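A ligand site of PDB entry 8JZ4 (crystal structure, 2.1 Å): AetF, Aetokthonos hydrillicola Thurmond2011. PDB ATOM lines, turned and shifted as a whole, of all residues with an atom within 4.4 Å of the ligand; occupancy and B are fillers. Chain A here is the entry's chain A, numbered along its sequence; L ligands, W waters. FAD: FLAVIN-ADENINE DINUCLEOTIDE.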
ATOM      1  N   ILE A  18      -7.296  12.201  17.671  1.00  0.00           N
ATOM      2  CA  ILE A  18      -6.282  11.966  16.602  1.00  0.00           C
ATOM      3  C   ILE A  18      -6.927  12.247  15.230  1.00  0.00           C
ATOM      4  O   ILE A  18      -7.867  11.576  14.827  1.00  0.00           O
ATOM      5  CB  ILE A  18      -5.667  10.569  16.728  1.00  0.00           C
ATOM      6  CG1 ILE A  18      -4.952  10.409  18.081  1.00  0.00           C
ATOM      7  CG2 ILE A  18      -4.756  10.267  15.549  1.00  0.00           C
ATOM      8  CD1 ILE A  18      -4.710   8.971  18.506  1.00  0.00           C
ATOM      9  N   GLY A  19      -6.412  13.258  14.565  1.00  0.00           N
ATOM     10  CA  GLY A  19      -6.881  13.692  13.253  1.00  0.00           C
ATOM     11  C   GLY A  19      -7.919  14.766  13.393  1.00  0.00           C
ATOM     12  O   GLY A  19      -8.878  14.571  14.192  1.00  0.00           O
ATOM     13  N   PHE A  20      -7.749  15.835  12.636  1.00  0.00           N
ATOM     14  CA  PHE A  20      -8.650  17.013  12.638  1.00  0.00           C
ATOM     15  C   PHE A  20      -8.848  17.492  11.223  1.00  0.00           C
ATOM     16  O   PHE A  20      -7.916  18.048  10.636  1.00  0.00           O
ATOM     17  CB  PHE A  20      -8.073  18.130  13.496  1.00  0.00           C
ATOM     18  CG  PHE A  20      -9.069  19.229  13.736  1.00  0.00           C
ATOM     19  CD1 PHE A  20     -10.004  19.130  14.747  1.00  0.00           C
ATOM     20  CD2 PHE A  20      -9.123  20.329  12.897  1.00  0.00           C
ATOM     21  CE1 PHE A  20     -10.920  20.143  14.962  1.00  0.00           C
ATOM     22  CE2 PHE A  20     -10.064  21.325  13.096  1.00  0.00           C
ATOM     23  CZ  PHE A  20     -10.961  21.229  14.140  1.00  0.00           C
ATOM     24  N   GLY A  21     -10.023  17.208  10.652  1.00  0.00           N
ATOM     25  CA  GLY A  21     -10.437  17.745   9.348  1.00  0.00           C
ATOM     26  C   GLY A  21     -11.825  18.336   9.401  1.00  0.00           C
ATOM     27  O   GLY A  21     -11.972  19.595   9.493  1.00  0.00           O
ATOM     28  N   PHE A  22     -12.823  17.467   9.329  1.00  0.00           N
ATOM     29  CA  PHE A  22     -14.244  17.868   9.260  1.00  0.00           C
ATOM     30  C   PHE A  22     -15.023  17.135  10.357  1.00  0.00           C
ATOM     31  O   PHE A  22     -15.859  17.761  11.050  1.00  0.00           O
ATOM     32  CB  PHE A  22     -14.734  17.628   7.821  1.00  0.00           C
ATOM     33  CG  PHE A  22     -16.233  17.628   7.708  1.00  0.00           C
ATOM     34  CD1 PHE A  22     -16.945  18.809   7.766  1.00  0.00           C
ATOM     35  CD2 PHE A  22     -16.921  16.430   7.605  1.00  0.00           C
ATOM     36  CE1 PHE A  22     -18.323  18.792   7.722  1.00  0.00           C
ATOM     37  CE2 PHE A  22     -18.296  16.423   7.525  1.00  0.00           C
ATOM     38  CZ  PHE A  22     -18.999  17.600   7.585  1.00  0.00           C
ATOM     39  N   SER A  23     -14.746  15.841  10.535  1.00  0.00           N
ATOM     40  CA  SER A  23     -15.536  14.923  11.390  1.00  0.00           C
ATOM     41  C   SER A  23     -15.415  15.335  12.863  1.00  0.00           C
ATOM     42  O   SER A  23     -16.360  15.152  13.583  1.00  0.00           O
ATOM     43  CB  SER A  23     -15.095  13.502  11.179  1.00  0.00           C
ATOM     44  OG  SER A  23     -15.455  13.050   9.875  1.00  0.00           O
ATOM     45  N   ILE A  41      -4.128  15.902  18.067  1.00  0.00           N
ATOM     46  CA  ILE A  41      -2.932  15.586  17.248  1.00  0.00           C
ATOM     47  C   ILE A  41      -3.386  15.348  15.800  1.00  0.00           C
ATOM     48  O   ILE A  41      -4.332  14.552  15.607  1.00  0.00           O
ATOM     49  CB  ILE A  41      -2.211  14.345  17.815  1.00  0.00           C
ATOM     50  CG1 ILE A  41      -1.911  14.491  19.308  1.00  0.00           C
ATOM     51  CG2 ILE A  41      -0.962  14.050  17.003  1.00  0.00           C
ATOM     52  CD1 ILE A  41      -1.328  13.248  19.931  1.00  0.00           C
ATOM     53  N   SER A  42      -2.759  16.021  14.845  1.00  0.00           N
ATOM     54  CA  SER A  42      -3.168  15.967  13.415  1.00  0.00           C
ATOM     55  C   SER A  42      -1.969  16.325  12.529  1.00  0.00           C
ATOM     56  O   SER A  42      -1.193  17.231  12.881  1.00  0.00           O
ATOM     57  CB  SER A  42      -4.359  16.857  13.163  1.00  0.00           C
ATOM     58  OG  SER A  42      -5.132  16.401  12.066  1.00  0.00           O
ATOM     59  N   ALA A  43      -1.803  15.582  11.431  1.00  0.00           N
ATOM     60  CA  ALA A  43      -0.618  15.600  10.536  1.00  0.00           C
ATOM     61  C   ALA A  43      -0.429  16.993   9.924  1.00  0.00           C
ATOM     62  O   ALA A  43      -1.423  17.611   9.566  1.00  0.00           O
ATOM     63  CB  ALA A  43      -0.775  14.557   9.477  1.00  0.00           C
ATOM     64  N   SER A  45       0.614  17.537   7.018  1.00  0.00           N
ATOM     65  CA  SER A  45       0.270  17.375   5.581  1.00  0.00           C
ATOM     66  C   SER A  45      -1.218  17.676   5.331  1.00  0.00           C
ATOM     67  O   SER A  45      -1.540  17.960   4.153  1.00  0.00           O
ATOM     68  CB  SER A  45       0.621  15.995   5.079  1.00  0.00           C
ATOM     69  OG  SER A  45      -0.410  15.065   5.394  1.00  0.00           O
ATOM     70  N   GLY A  46      -2.090  17.591   6.341  1.00  0.00           N
ATOM     71  CA  GLY A  46      -3.548  17.768   6.151  1.00  0.00           C
ATOM     72  C   GLY A  46      -4.158  16.644   5.326  1.00  0.00           C
ATOM     73  O   GLY A  46      -3.736  15.497   5.501  1.00  0.00           O
ATOM     74  N   SER A  47      -5.109  16.934   4.432  1.00  0.00           N
ATOM     75  CA  SER A  47      -6.021  15.923   3.808  1.00  0.00           C
ATOM     76  C   SER A  47      -6.052  16.036   2.279  1.00  0.00           C
ATOM     77  O   SER A  47      -5.228  16.785   1.707  1.00  0.00           O
ATOM     78  CB  SER A  47      -7.398  16.044   4.367  1.00  0.00           C
ATOM     79  OG  SER A  47      -8.061  17.189   3.851  1.00  0.00           O
ATOM     80  N   VAL A  48      -6.974  15.275   1.644  1.00  0.00           N
ATOM     81  CA  VAL A  48      -7.295  15.355   0.191  1.00  0.00           C
ATOM     82  C   VAL A  48      -7.508  16.834  -0.141  1.00  0.00           C
ATOM     83  O   VAL A  48      -6.975  17.308  -1.166  1.00  0.00           O
ATOM     84  CB  VAL A  48      -8.569  14.587  -0.221  1.00  0.00           C
ATOM     85  CG1 VAL A  48      -8.392  13.906  -1.567  1.00  0.00           C
ATOM     86  CG2 VAL A  48      -9.065  13.602   0.823  1.00  0.00           C
ATOM     87  N   TRP A  49      -8.271  17.533   0.702  1.00  0.00           N
ATOM     88  CA  TRP A  49      -8.818  18.876   0.388  1.00  0.00           C
ATOM     89  C   TRP A  49      -7.655  19.862   0.233  1.00  0.00           C
ATOM     90  O   TRP A  49      -7.794  20.768  -0.613  1.00  0.00           O
ATOM     91  CB  TRP A  49      -9.857  19.316   1.428  1.00  0.00           C
ATOM     92  CG  TRP A  49     -11.021  18.370   1.525  1.00  0.00           C
ATOM     93  CD1 TRP A  49     -11.196  17.387   2.452  1.00  0.00           C
ATOM     94  CD2 TRP A  49     -12.162  18.294   0.651  1.00  0.00           C
ATOM     95  NE1 TRP A  49     -12.357  16.714   2.216  1.00  0.00           N
ATOM     96  CE2 TRP A  49     -12.972  17.240   1.116  1.00  0.00           C
ATOM     97  CE3 TRP A  49     -12.583  19.014  -0.478  1.00  0.00           C
ATOM     98  CZ2 TRP A  49     -14.174  16.896   0.503  1.00  0.00           C
ATOM     99  CZ3 TRP A  49     -13.766  18.659  -1.096  1.00  0.00           C
ATOM    100  CH2 TRP A  49     -14.561  17.632  -0.597  1.00  0.00           C
ATOM    101  N   PHE A  60     -15.374  21.551  -8.188  1.00  0.00           N
ATOM    102  CA  PHE A  60     -16.596  20.711  -8.213  1.00  0.00           C
ATOM    103  C   PHE A  60     -17.477  21.149  -7.041  1.00  0.00           C
ATOM    104  O   PHE A  60     -17.129  22.100  -6.330  1.00  0.00           O
ATOM    105  CB  PHE A  60     -16.242  19.231  -8.182  1.00  0.00           C
ATOM    106  CG  PHE A  60     -15.436  18.754  -6.990  1.00  0.00           C
ATOM    107  CD1 PHE A  60     -14.065  18.971  -6.927  1.00  0.00           C
ATOM    108  CD2 PHE A  60     -16.041  18.046  -5.965  1.00  0.00           C
ATOM    109  CE1 PHE A  60     -13.324  18.515  -5.845  1.00  0.00           C
ATOM    110  CE2 PHE A  60     -15.299  17.586  -4.892  1.00  0.00           C
ATOM    111  CZ  PHE A  60     -13.942  17.822  -4.828  1.00  0.00           C
ATOM    112  N   LEU A  62     -20.508  19.673  -3.859  1.00  0.00           N
ATOM    113  CA  LEU A  62     -20.999  18.490  -3.104  1.00  0.00           C
ATOM    114  C   LEU A  62     -22.210  17.907  -3.841  1.00  0.00           C
ATOM    115  O   LEU A  62     -22.973  18.672  -4.410  1.00  0.00           O
ATOM    116  CB  LEU A  62     -21.368  18.912  -1.672  1.00  0.00           C
ATOM    117  CG  LEU A  62     -20.253  19.610  -0.891  1.00  0.00           C
ATOM    118  CD1 LEU A  62     -20.632  19.772   0.566  1.00  0.00           C
ATOM    119  CD2 LEU A  62     -18.936  18.865  -1.018  1.00  0.00           C
ATOM    120  N   VAL A  63     -22.416  16.596  -3.735  1.00  0.00           N
ATOM    121  CA  VAL A  63     -23.649  15.862  -4.156  1.00  0.00           C
ATOM    122  C   VAL A  63     -24.767  16.068  -3.127  1.00  0.00           C
ATOM    123  O   VAL A  63     -25.931  15.705  -3.430  1.00  0.00           O
ATOM    124  CB  VAL A  63     -23.337  14.359  -4.356  1.00  0.00           C
ATOM    125  CG1 VAL A  63     -22.178  14.130  -5.320  1.00  0.00           C
ATOM    126  CG2 VAL A  63     -23.040  13.631  -3.063  1.00  0.00           C
ATOM    127  N   SER A  64     -24.459  16.676  -1.964  1.00  0.00           N
ATOM    128  CA  SER A  64     -25.387  16.799  -0.813  1.00  0.00           C
ATOM    129  C   SER A  64     -25.770  18.263  -0.528  1.00  0.00           C
ATOM    130  O   SER A  64     -24.955  19.162  -0.750  1.00  0.00           O
ATOM    131  CB  SER A  64     -24.791  16.152   0.419  1.00  0.00           C
ATOM    132  OG  SER A  64     -23.486  16.664   0.652  1.00  0.00           O
ATOM    133  N   SER A  69     -24.873  18.861   5.157  1.00  0.00           N
ATOM    134  CA  SER A  69     -23.414  18.827   4.872  1.00  0.00           C
ATOM    135  C   SER A  69     -22.608  19.776   5.769  1.00  0.00           C
ATOM    136  O   SER A  69     -21.376  19.703   5.740  1.00  0.00           O
ATOM    137  CB  SER A  69     -23.174  19.082   3.415  1.00  0.00           C
ATOM    138  OG  SER A  69     -23.934  18.166   2.616  1.00  0.00           O
ATOM    139  N   PHE A  90     -16.874  24.186   1.085  1.00  0.00           N
ATOM    140  CA  PHE A  90     -16.669  23.079   2.067  1.00  0.00           C
ATOM    141  C   PHE A  90     -15.276  23.214   2.712  1.00  0.00           C
ATOM    142  O   PHE A  90     -15.137  23.269   3.969  1.00  0.00           O
ATOM    143  CB  PHE A  90     -16.911  21.746   1.372  1.00  0.00           C
ATOM    144  CG  PHE A  90     -17.187  20.573   2.279  1.00  0.00           C
ATOM    145  CD1 PHE A  90     -18.135  20.646   3.287  1.00  0.00           C
ATOM    146  CD2 PHE A  90     -16.520  19.373   2.096  1.00  0.00           C
ATOM    147  CE1 PHE A  90     -18.372  19.568   4.117  1.00  0.00           C
ATOM    148  CE2 PHE A  90     -16.783  18.279   2.909  1.00  0.00           C
ATOM    149  CZ  PHE A  90     -17.722  18.368   3.911  1.00  0.00           C
ATOM    150  N   ASP A 108       1.562  16.561  14.285  1.00  0.00           N
ATOM    151  CA  ASP A 108       2.365  15.327  14.351  1.00  0.00           C
ATOM    152  C   ASP A 108       1.531  14.184  13.806  1.00  0.00           C
ATOM    153  O   ASP A 108       0.299  14.360  13.656  1.00  0.00           O
ATOM    154  CB  ASP A 108       2.819  15.026  15.781  1.00  0.00           C
ATOM    155  CG  ASP A 108       4.146  14.290  15.898  1.00  0.00           C
ATOM    156  OD1 ASP A 108       4.622  13.704  14.871  1.00  0.00           O
ATOM    157  OD2 ASP A 108       4.702  14.302  17.022  1.00  0.00           O
ATOM    158  N   PHE A 109       2.183  13.061  13.549  1.00  0.00           N
ATOM    159  CA  PHE A 109       1.566  11.878  12.918  1.00  0.00           C
ATOM    160  C   PHE A 109       1.610  10.721  13.919  1.00  0.00           C
ATOM    161  O   PHE A 109       2.699  10.341  14.320  1.00  0.00           O
ATOM    162  CB  PHE A 109       2.231  11.569  11.583  1.00  0.00           C
ATOM    163  CG  PHE A 109       1.556  10.435  10.864  1.00  0.00           C
ATOM    164  CD1 PHE A 109       0.385  10.653  10.143  1.00  0.00           C
ATOM    165  CD2 PHE A 109       2.045   9.142  10.962  1.00  0.00           C
ATOM    166  CE1 PHE A 109      -0.253   9.601   9.513  1.00  0.00           C
ATOM    167  CE2 PHE A 109       1.385   8.090  10.331  1.00  0.00           C
ATOM    168  CZ  PHE A 109       0.244   8.329   9.614  1.00  0.00           C
ATOM    169  N   VAL A 110       0.448  10.164  14.251  1.00  0.00           N
ATOM    170  CA  VAL A 110       0.362   9.061  15.242  1.00  0.00           C
ATOM    171  C   VAL A 110       0.652   7.757  14.490  1.00  0.00           C
ATOM    172  O   VAL A 110      -0.013   7.463  13.479  1.00  0.00           O
ATOM    173  CB  VAL A 110      -0.982   9.043  15.965  1.00  0.00           C
ATOM    174  CG1 VAL A 110      -1.166   7.783  16.794  1.00  0.00           C
ATOM    175  CG2 VAL A 110      -1.151  10.289  16.802  1.00  0.00           C
ATOM    176  N   ALA A 138     -10.380  10.263  14.362  1.00  0.00           N
ATOM    177  CA  ALA A 138     -11.122  11.023  13.333  1.00  0.00           C
ATOM    178  C   ALA A 138     -10.177  11.245  12.146  1.00  0.00           C
ATOM    179  O   ALA A 138     -10.026  12.400  11.710  1.00  0.00           O
ATOM    180  CB  ALA A 138     -11.642  12.318  13.910  1.00  0.00           C
ATOM    181  N   THR A 139      -9.591  10.148  11.659  1.00  0.00           N
ATOM    182  CA  THR A 139      -8.459  10.136  10.696  1.00  0.00           C
ATOM    183  C   THR A 139      -8.937   9.970   9.251  1.00  0.00           C
ATOM    184  O   THR A 139      -8.094  10.050   8.349  1.00  0.00           O
ATOM    185  CB  THR A 139      -7.448   9.037  11.027  1.00  0.00           C
ATOM    186  OG1 THR A 139      -8.182   7.814  11.155  1.00  0.00           O
ATOM    187  CG2 THR A 139      -6.651   9.355  12.275  1.00  0.00           C
ATOM    188  N   GLY A 140     -10.229   9.732   9.009  1.00  0.00           N
ATOM    189  CA  GLY A 140     -10.740   9.612   7.641  1.00  0.00           C
ATOM    190  C   GLY A 140     -10.289   8.329   6.958  1.00  0.00           C
ATOM    191  O   GLY A 140      -9.867   7.380   7.669  1.00  0.00           O
ATOM    192  N   ARG A 143      -8.371   6.717   0.007  1.00  0.00           N
ATOM    193  CA  ARG A 143      -9.232   6.464  -1.185  1.00  0.00           C
ATOM    194  C   ARG A 143      -8.361   6.424  -2.459  1.00  0.00           C
ATOM    195  O   ARG A 143      -7.760   7.475  -2.810  1.00  0.00           O
ATOM    196  CB  ARG A 143     -10.328   7.517  -1.300  1.00  0.00           C
ATOM    197  CG  ARG A 143     -11.657   7.053  -0.715  1.00  0.00           C
ATOM    198  CD  ARG A 143     -12.746   8.088  -0.801  1.00  0.00           C
ATOM    199  NE  ARG A 143     -13.617   7.931   0.344  1.00  0.00           N
ATOM    200  CZ  ARG A 143     -13.710   8.777   1.375  1.00  0.00           C
ATOM    201  NH1 ARG A 143     -14.537   8.509   2.373  1.00  0.00           N
ATOM    202  NH2 ARG A 143     -12.998   9.893   1.415  1.00  0.00           N
ATOM    203  N   ASN A 146      -8.552   9.169  -5.215  1.00  0.00           N
ATOM    204  CA  ASN A 146      -8.172  10.568  -4.869  1.00  0.00           C
ATOM    205  C   ASN A 146      -7.070  11.049  -5.821  1.00  0.00           C
ATOM    206  O   ASN A 146      -7.093  12.251  -6.149  1.00  0.00           O
ATOM    207  CB  ASN A 146      -7.808  10.724  -3.386  1.00  0.00           C
ATOM    208  CG  ASN A 146      -9.017  10.692  -2.465  1.00  0.00           C
ATOM    209  OD1 ASN A 146     -10.161  10.852  -2.903  1.00  0.00           O
ATOM    210  ND2 ASN A 146      -8.767  10.508  -1.181  1.00  0.00           N
ATOM    211  N   LEU A 149      -8.339  12.510  -9.118  1.00  0.00           N
ATOM    212  CA  LEU A 149      -8.900  13.855  -8.832  1.00  0.00           C
ATOM    213  C   LEU A 149      -7.741  14.829  -8.585  1.00  0.00           C
ATOM    214  O   LEU A 149      -7.736  15.896  -9.224  1.00  0.00           O
ATOM    215  CB  LEU A 149      -9.839  13.779  -7.627  1.00  0.00           C
ATOM    216  CG  LEU A 149     -10.963  12.748  -7.710  1.00  0.00           C
ATOM    217  CD1 LEU A 149     -11.731  12.666  -6.392  1.00  0.00           C
ATOM    218  CD2 LEU A 149     -11.919  13.034  -8.861  1.00  0.00           C
ATOM    219  N   ARG A 343      -8.120   5.043   7.880  1.00  0.00           N
ATOM    220  CA  ARG A 343      -6.694   5.356   8.167  1.00  0.00           C
ATOM    221  C   ARG A 343      -6.455   5.196   9.677  1.00  0.00           C
ATOM    222  O   ARG A 343      -6.254   6.199  10.347  1.00  0.00           O
ATOM    223  CB  ARG A 343      -6.348   6.776   7.739  1.00  0.00           C
ATOM    224  CG  ARG A 343      -5.551   6.865   6.453  1.00  0.00           C
ATOM    225  CD  ARG A 343      -5.033   8.272   6.216  1.00  0.00           C
ATOM    226  NE  ARG A 343      -6.144   9.211   6.090  1.00  0.00           N
ATOM    227  CZ  ARG A 343      -6.000  10.507   5.846  1.00  0.00           C
ATOM    228  NH1 ARG A 343      -7.071  11.288   5.774  1.00  0.00           N
ATOM    229  NH2 ARG A 343      -4.790  11.012   5.677  1.00  0.00           N
ATOM    230  N   ARG A 381     -20.674   5.998   6.754  1.00  0.00           N
ATOM    231  CA  ARG A 381     -20.997   6.746   5.514  1.00  0.00           C
ATOM    232  C   ARG A 381     -22.509   6.779   5.376  1.00  0.00           C
ATOM    233  O   ARG A 381     -23.151   5.753   5.532  1.00  0.00           O
ATOM    234  CB  ARG A 381     -20.384   6.092   4.266  1.00  0.00           C
ATOM    235  CG  ARG A 381     -18.867   6.084   4.244  1.00  0.00           C
ATOM    236  CD  ARG A 381     -18.247   7.146   3.341  1.00  0.00           C
ATOM    237  NE  ARG A 381     -17.126   7.889   3.955  1.00  0.00           N
ATOM    238  CZ  ARG A 381     -17.098   9.213   4.229  1.00  0.00           C
ATOM    239  NH1 ARG A 381     -18.136   9.973   3.941  1.00  0.00           N
ATOM    240  NH2 ARG A 381     -16.017   9.753   4.778  1.00  0.00           N
ATOM    241  N   GLY A 386     -25.248  14.552   3.230  1.00  0.00           N
ATOM    242  CA  GLY A 386     -23.834  14.749   3.540  1.00  0.00           C
ATOM    243  C   GLY A 386     -23.461  14.040   4.833  1.00  0.00           C
ATOM    244  O   GLY A 386     -24.400  13.625   5.611  1.00  0.00           O
ATOM    245  N   LEU A 387     -22.162  13.971   5.087  1.00  0.00           N
ATOM    246  CA  LEU A 387     -21.539  13.295   6.245  1.00  0.00           C
ATOM    247  C   LEU A 387     -21.861  14.065   7.524  1.00  0.00           C
ATOM    248  O   LEU A 387     -22.025  13.383   8.583  1.00  0.00           O
ATOM    249  CB  LEU A 387     -20.028  13.224   6.000  1.00  0.00           C
ATOM    250  CG  LEU A 387     -19.214  12.576   7.119  1.00  0.00           C
ATOM    251  CD1 LEU A 387     -19.661  11.131   7.323  1.00  0.00           C
ATOM    252  CD2 LEU A 387     -17.722  12.644   6.840  1.00  0.00           C
HETATM  253  PA  FAD L   1     -10.200  14.167   6.679  1.00  0.00           P
HETATM  254  O1A FAD L   1     -10.881  15.380   6.125  1.00  0.00           O
HETATM  255  O2A FAD L   1      -9.402  13.347   5.745  1.00  0.00           O
HETATM  256  O5B FAD L   1      -9.298  14.636   7.909  1.00  0.00           O
HETATM  257  C5B FAD L   1      -8.522  13.693   8.699  1.00  0.00           C
HETATM  258  C4B FAD L   1      -7.235  14.334   9.139  1.00  0.00           C
HETATM  259  O4B FAD L   1      -6.527  13.402   9.995  1.00  0.00           O
HETATM  260  C3B FAD L   1      -6.243  14.690   8.001  1.00  0.00           C
HETATM  261  O3B FAD L   1      -5.671  15.974   8.138  1.00  0.00           O
HETATM  262  C2B FAD L   1      -5.097  13.677   8.169  1.00  0.00           C
HETATM  263  O2B FAD L   1      -3.824  14.195   7.860  1.00  0.00           O
HETATM  264  C1B FAD L   1      -5.150  13.380   9.656  1.00  0.00           C
HETATM  265  N9A FAD L   1      -4.575  12.077  10.022  1.00  0.00           N
HETATM  266  C8A FAD L   1      -4.852  10.829   9.485  1.00  0.00           C
HETATM  267  N7A FAD L   1      -4.199   9.866  10.101  1.00  0.00           N
HETATM  268  C5A FAD L   1      -3.449  10.504  11.072  1.00  0.00           C
HETATM  269  C6A FAD L   1      -2.554  10.036  12.052  1.00  0.00           C
HETATM  270  N6A FAD L   1      -2.245   8.760  12.226  1.00  0.00           N
HETATM  271  N1A FAD L   1      -1.987  10.951  12.858  1.00  0.00           N
HETATM  272  C2A FAD L   1      -2.301  12.247  12.698  1.00  0.00           C
HETATM  273  N3A FAD L   1      -3.126  12.813  11.835  1.00  0.00           N
HETATM  274  C4A FAD L   1      -3.675  11.869  11.042  1.00  0.00           C
HETATM  275  N1  FAD L   1     -19.123  14.375   2.074  1.00  0.00           N
HETATM  276  C2  FAD L   1     -20.303  15.006   1.944  1.00  0.00           C
HETATM  277  O2  FAD L   1     -21.051  15.119   2.898  1.00  0.00           O
HETATM  278  N3  FAD L   1     -20.755  15.495   0.753  1.00  0.00           N
HETATM  279  C4  FAD L   1     -19.986  15.446  -0.396  1.00  0.00           C
HETATM  280  O4  FAD L   1     -20.426  15.876  -1.467  1.00  0.00           O
HETATM  281  C4X FAD L   1     -18.707  14.851  -0.284  1.00  0.00           C
HETATM  282  N5  FAD L   1     -17.944  14.831  -1.358  1.00  0.00           N
HETATM  283  C5X FAD L   1     -16.699  14.296  -1.228  1.00  0.00           C
HETATM  284  C6  FAD L   1     -15.853  14.309  -2.352  1.00  0.00           C
HETATM  285  C7  FAD L   1     -14.583  13.796  -2.326  1.00  0.00           C
HETATM  286  C7M FAD L   1     -13.726  13.823  -3.562  1.00  0.00           C
HETATM  287  C8  FAD L   1     -14.101  13.220  -1.098  1.00  0.00           C
HETATM  288  C8M FAD L   1     -12.713  12.630  -1.012  1.00  0.00           C
HETATM  289  C9  FAD L   1     -14.936  13.172   0.008  1.00  0.00           C
HETATM  290  C9A FAD L   1     -16.238  13.716  -0.011  1.00  0.00           C
HETATM  291  N10 FAD L   1     -17.076  13.745   1.108  1.00  0.00           N
HETATM  292  C10 FAD L   1     -18.334  14.322   1.015  1.00  0.00           C
HETATM  293  C1' FAD L   1     -16.721  13.013   2.343  1.00  0.00           C
HETATM  294  C2' FAD L   1     -16.268  13.799   3.556  1.00  0.00           C
HETATM  295  O2' FAD L   1     -17.062  14.961   3.777  1.00  0.00           O
HETATM  296  C3' FAD L   1     -14.771  14.104   3.454  1.00  0.00           C
HETATM  297  O3' FAD L   1     -14.096  12.881   3.152  1.00  0.00           O
HETATM  298  C4' FAD L   1     -14.133  14.654   4.719  1.00  0.00           C
HETATM  299  O4' FAD L   1     -12.874  15.238   4.405  1.00  0.00           O
HETATM  300  C5' FAD L   1     -13.870  13.611   5.767  1.00  0.00           C
HETATM  301  O5' FAD L   1     -13.491  14.346   6.962  1.00  0.00           O
HETATM  302  P   FAD L   1     -12.686  13.573   8.119  1.00  0.00           P
HETATM  303  O1P FAD L   1     -12.468  14.596   9.212  1.00  0.00           O
HETATM  304  O2P FAD L   1     -13.383  12.292   8.445  1.00  0.00           O
HETATM  305  O3P FAD L   1     -11.303  13.249   7.392  1.00  0.00           O
HETATM  306  O   HOH W   1     -18.629  15.832  -4.399  1.00  0.00           O
HETATM  307  O   HOH W   2     -12.702  10.490  10.335  1.00  0.00           O
HETATM  308  O   HOH W   3      -7.554  17.953   7.744  1.00  0.00           O
HETATM  309  O   HOH W   4     -14.097  10.116   7.191  1.00  0.00           O
HETATM  310  O   HOH W   5      -3.810   6.929  10.496  1.00  0.00           O
HETATM  311  O   HOH W   6     -11.507  14.961  11.734  1.00  0.00           O
HETATM  312  O   HOH W   7      -4.162  17.351   9.911  1.00  0.00           O
HETATM  313  O   HOH W   8     -20.985  16.924   5.192  1.00  0.00           O
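Water W4 bridges an oxygen (O2P) of the ligand and the guanidinium group of Arg 381.
Water W2 lies within hydrogen-bond range of O2P of the ligand (2.7 Å), N of Gly 140 (2.9 Å) and N of Thr 139 (3.4 Å).
Water W7 lies within hydrogen-bond range of the side-chain hydroxyl (OG) of Ser 42 (2.5 Å), an oxygen (O3B) of the ligand (2.7 Å) and the backbone carbonyl oxygen (O) of Ala 43 (2.8 Å).
Water W6 lies within hydrogen-bond range of O1P of the ligand, N of Gly 21 and O of Ala 138.
Water W3 bridges O3B of the ligand (2.8 Å) and O of Phe 20 (2.9 Å).
Water W5 lies within hydrogen-bond range of O of Arg 343 (2.6 Å) and N6A of the ligand (3.0 Å).
N of Ala 43 is in hydrogen-bond range of O of Asp 108, at 3.3 Å.
N of Gly 19 sits at hydrogen-bond distance from O of Ile 41.
The backbone NH (N) of Ala 138 is in hydrogen-bond range of the backbone carbonyl oxygen (O) of Ile 18, at 2.9 Å.
The backbone carbonyl oxygen (O) of Arg 343 lies within hydrogen-bond range of the side-chain hydroxyl (OG1) of Thr 139.
O of Gly 140 is in hydrogen-bond range of N of Arg 343, at 2.9 Å.
The side-chain hydroxyl of Ser 42 is in hydrogen-bond range of the backbone NH of Phe 20.
N of Asp 108 sits at hydrogen-bond distance from O of Ser 42 (3.2 Å).
OG of Ser 64 is in hydrogen-bond range of OG of Ser 69 (2.5 Å).
Ile 18 touches the ligand (CG2 to N1A, 3.9 Å).
Gly 19 touches the ligand (CA to O4B, 3.3 Å).
Phe 20 touches the ligand.
CA of Gly 21 touches O5B of the ligand, 3.6 Å away.
Ser 42 touches the ligand (CA to N3A, 3.5 Å).
Ser 47 touches the ligand.
Leu 62 touches the ligand (CA to O4, 3.1 Å).
CE2 of Phe 90 touches O2' of the ligand (3.4 Å).
O of Asp 108 touches C2A of the ligand, 3.5 Å away.
Phe 109 touches the ligand.
O of Ala 138 touches C5B of the ligand, 3.6 Å away.
Thr 139 touches the ligand (CG2 to N7A, 3.3 Å).
Gly 140 touches the ligand (CA to O3P, 3.7 Å).
NH2 of Arg 143 touches O3' of the ligand (3.6 Å).
Asn 146 touches the ligand.
CD1 of Leu 149 touches C7M of the ligand, 3.7 Å away.
Arg 381 touches the ligand (NH1 to C1', 3.7 Å).
Gly 386 touches the ligand (CA to O2, 2.9 Å).
Of the 33 residues printed, 28 come within 4 Å of the ligand.
The nearest printed residue that does not touch the ligand is Phe 60 (4.2 Å).
The side-chain hydroxyl of Ser 23 lies within hydrogen-bond range of an oxygen (O2P) of the ligand, at 2.6 Å.
The guanidinium group (NH1) of Arg 343 lies within salt-bridge range of an oxygen (O2A) of the ligand (3.1 Å).
NE1 of Trp 49 sits at hydrogen-bond distance from O4' of the ligand (2.7 Å).
A nitrogen (N6A) of the ligand sits at hydrogen-bond distance from the backbone carbonyl oxygen of Val 110 (2.9 Å).
The backbone NH (N) of Val 110 sits at hydrogen-bond distance from a nitrogen (N1A) of the ligand, at 2.9 Å.
The backbone NH (N) of Ser 23 sits at hydrogen-bond distance from an oxygen (O1P) of the ligand, 2.9 Å away.
N3A of the ligand lies within hydrogen-bond range of N of Ala 43, at 3.1 Å.
The backbone carbonyl oxygen (O) of Gly 46 lies within hydrogen-bond range of an oxygen (O2B) of the ligand, at 2.7 Å.
The side-chain hydroxyl (OG) of Ser 64 is in hydrogen-bond range of a nitrogen (N3) of the ligand (3.0 Å).
An oxygen (O1P) of the ligand lies within hydrogen-bond range of the backbone NH (N) of Phe 22, at 2.9 Å.
The backbone NH (N) of Val 63 is in hydrogen-bond range of an oxygen (O4) of the ligand, at 3.1 Å.
An oxygen (O2) of the ligand lies within hydrogen-bond range of the backbone NH (N) of Leu 387 (2.7 Å).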
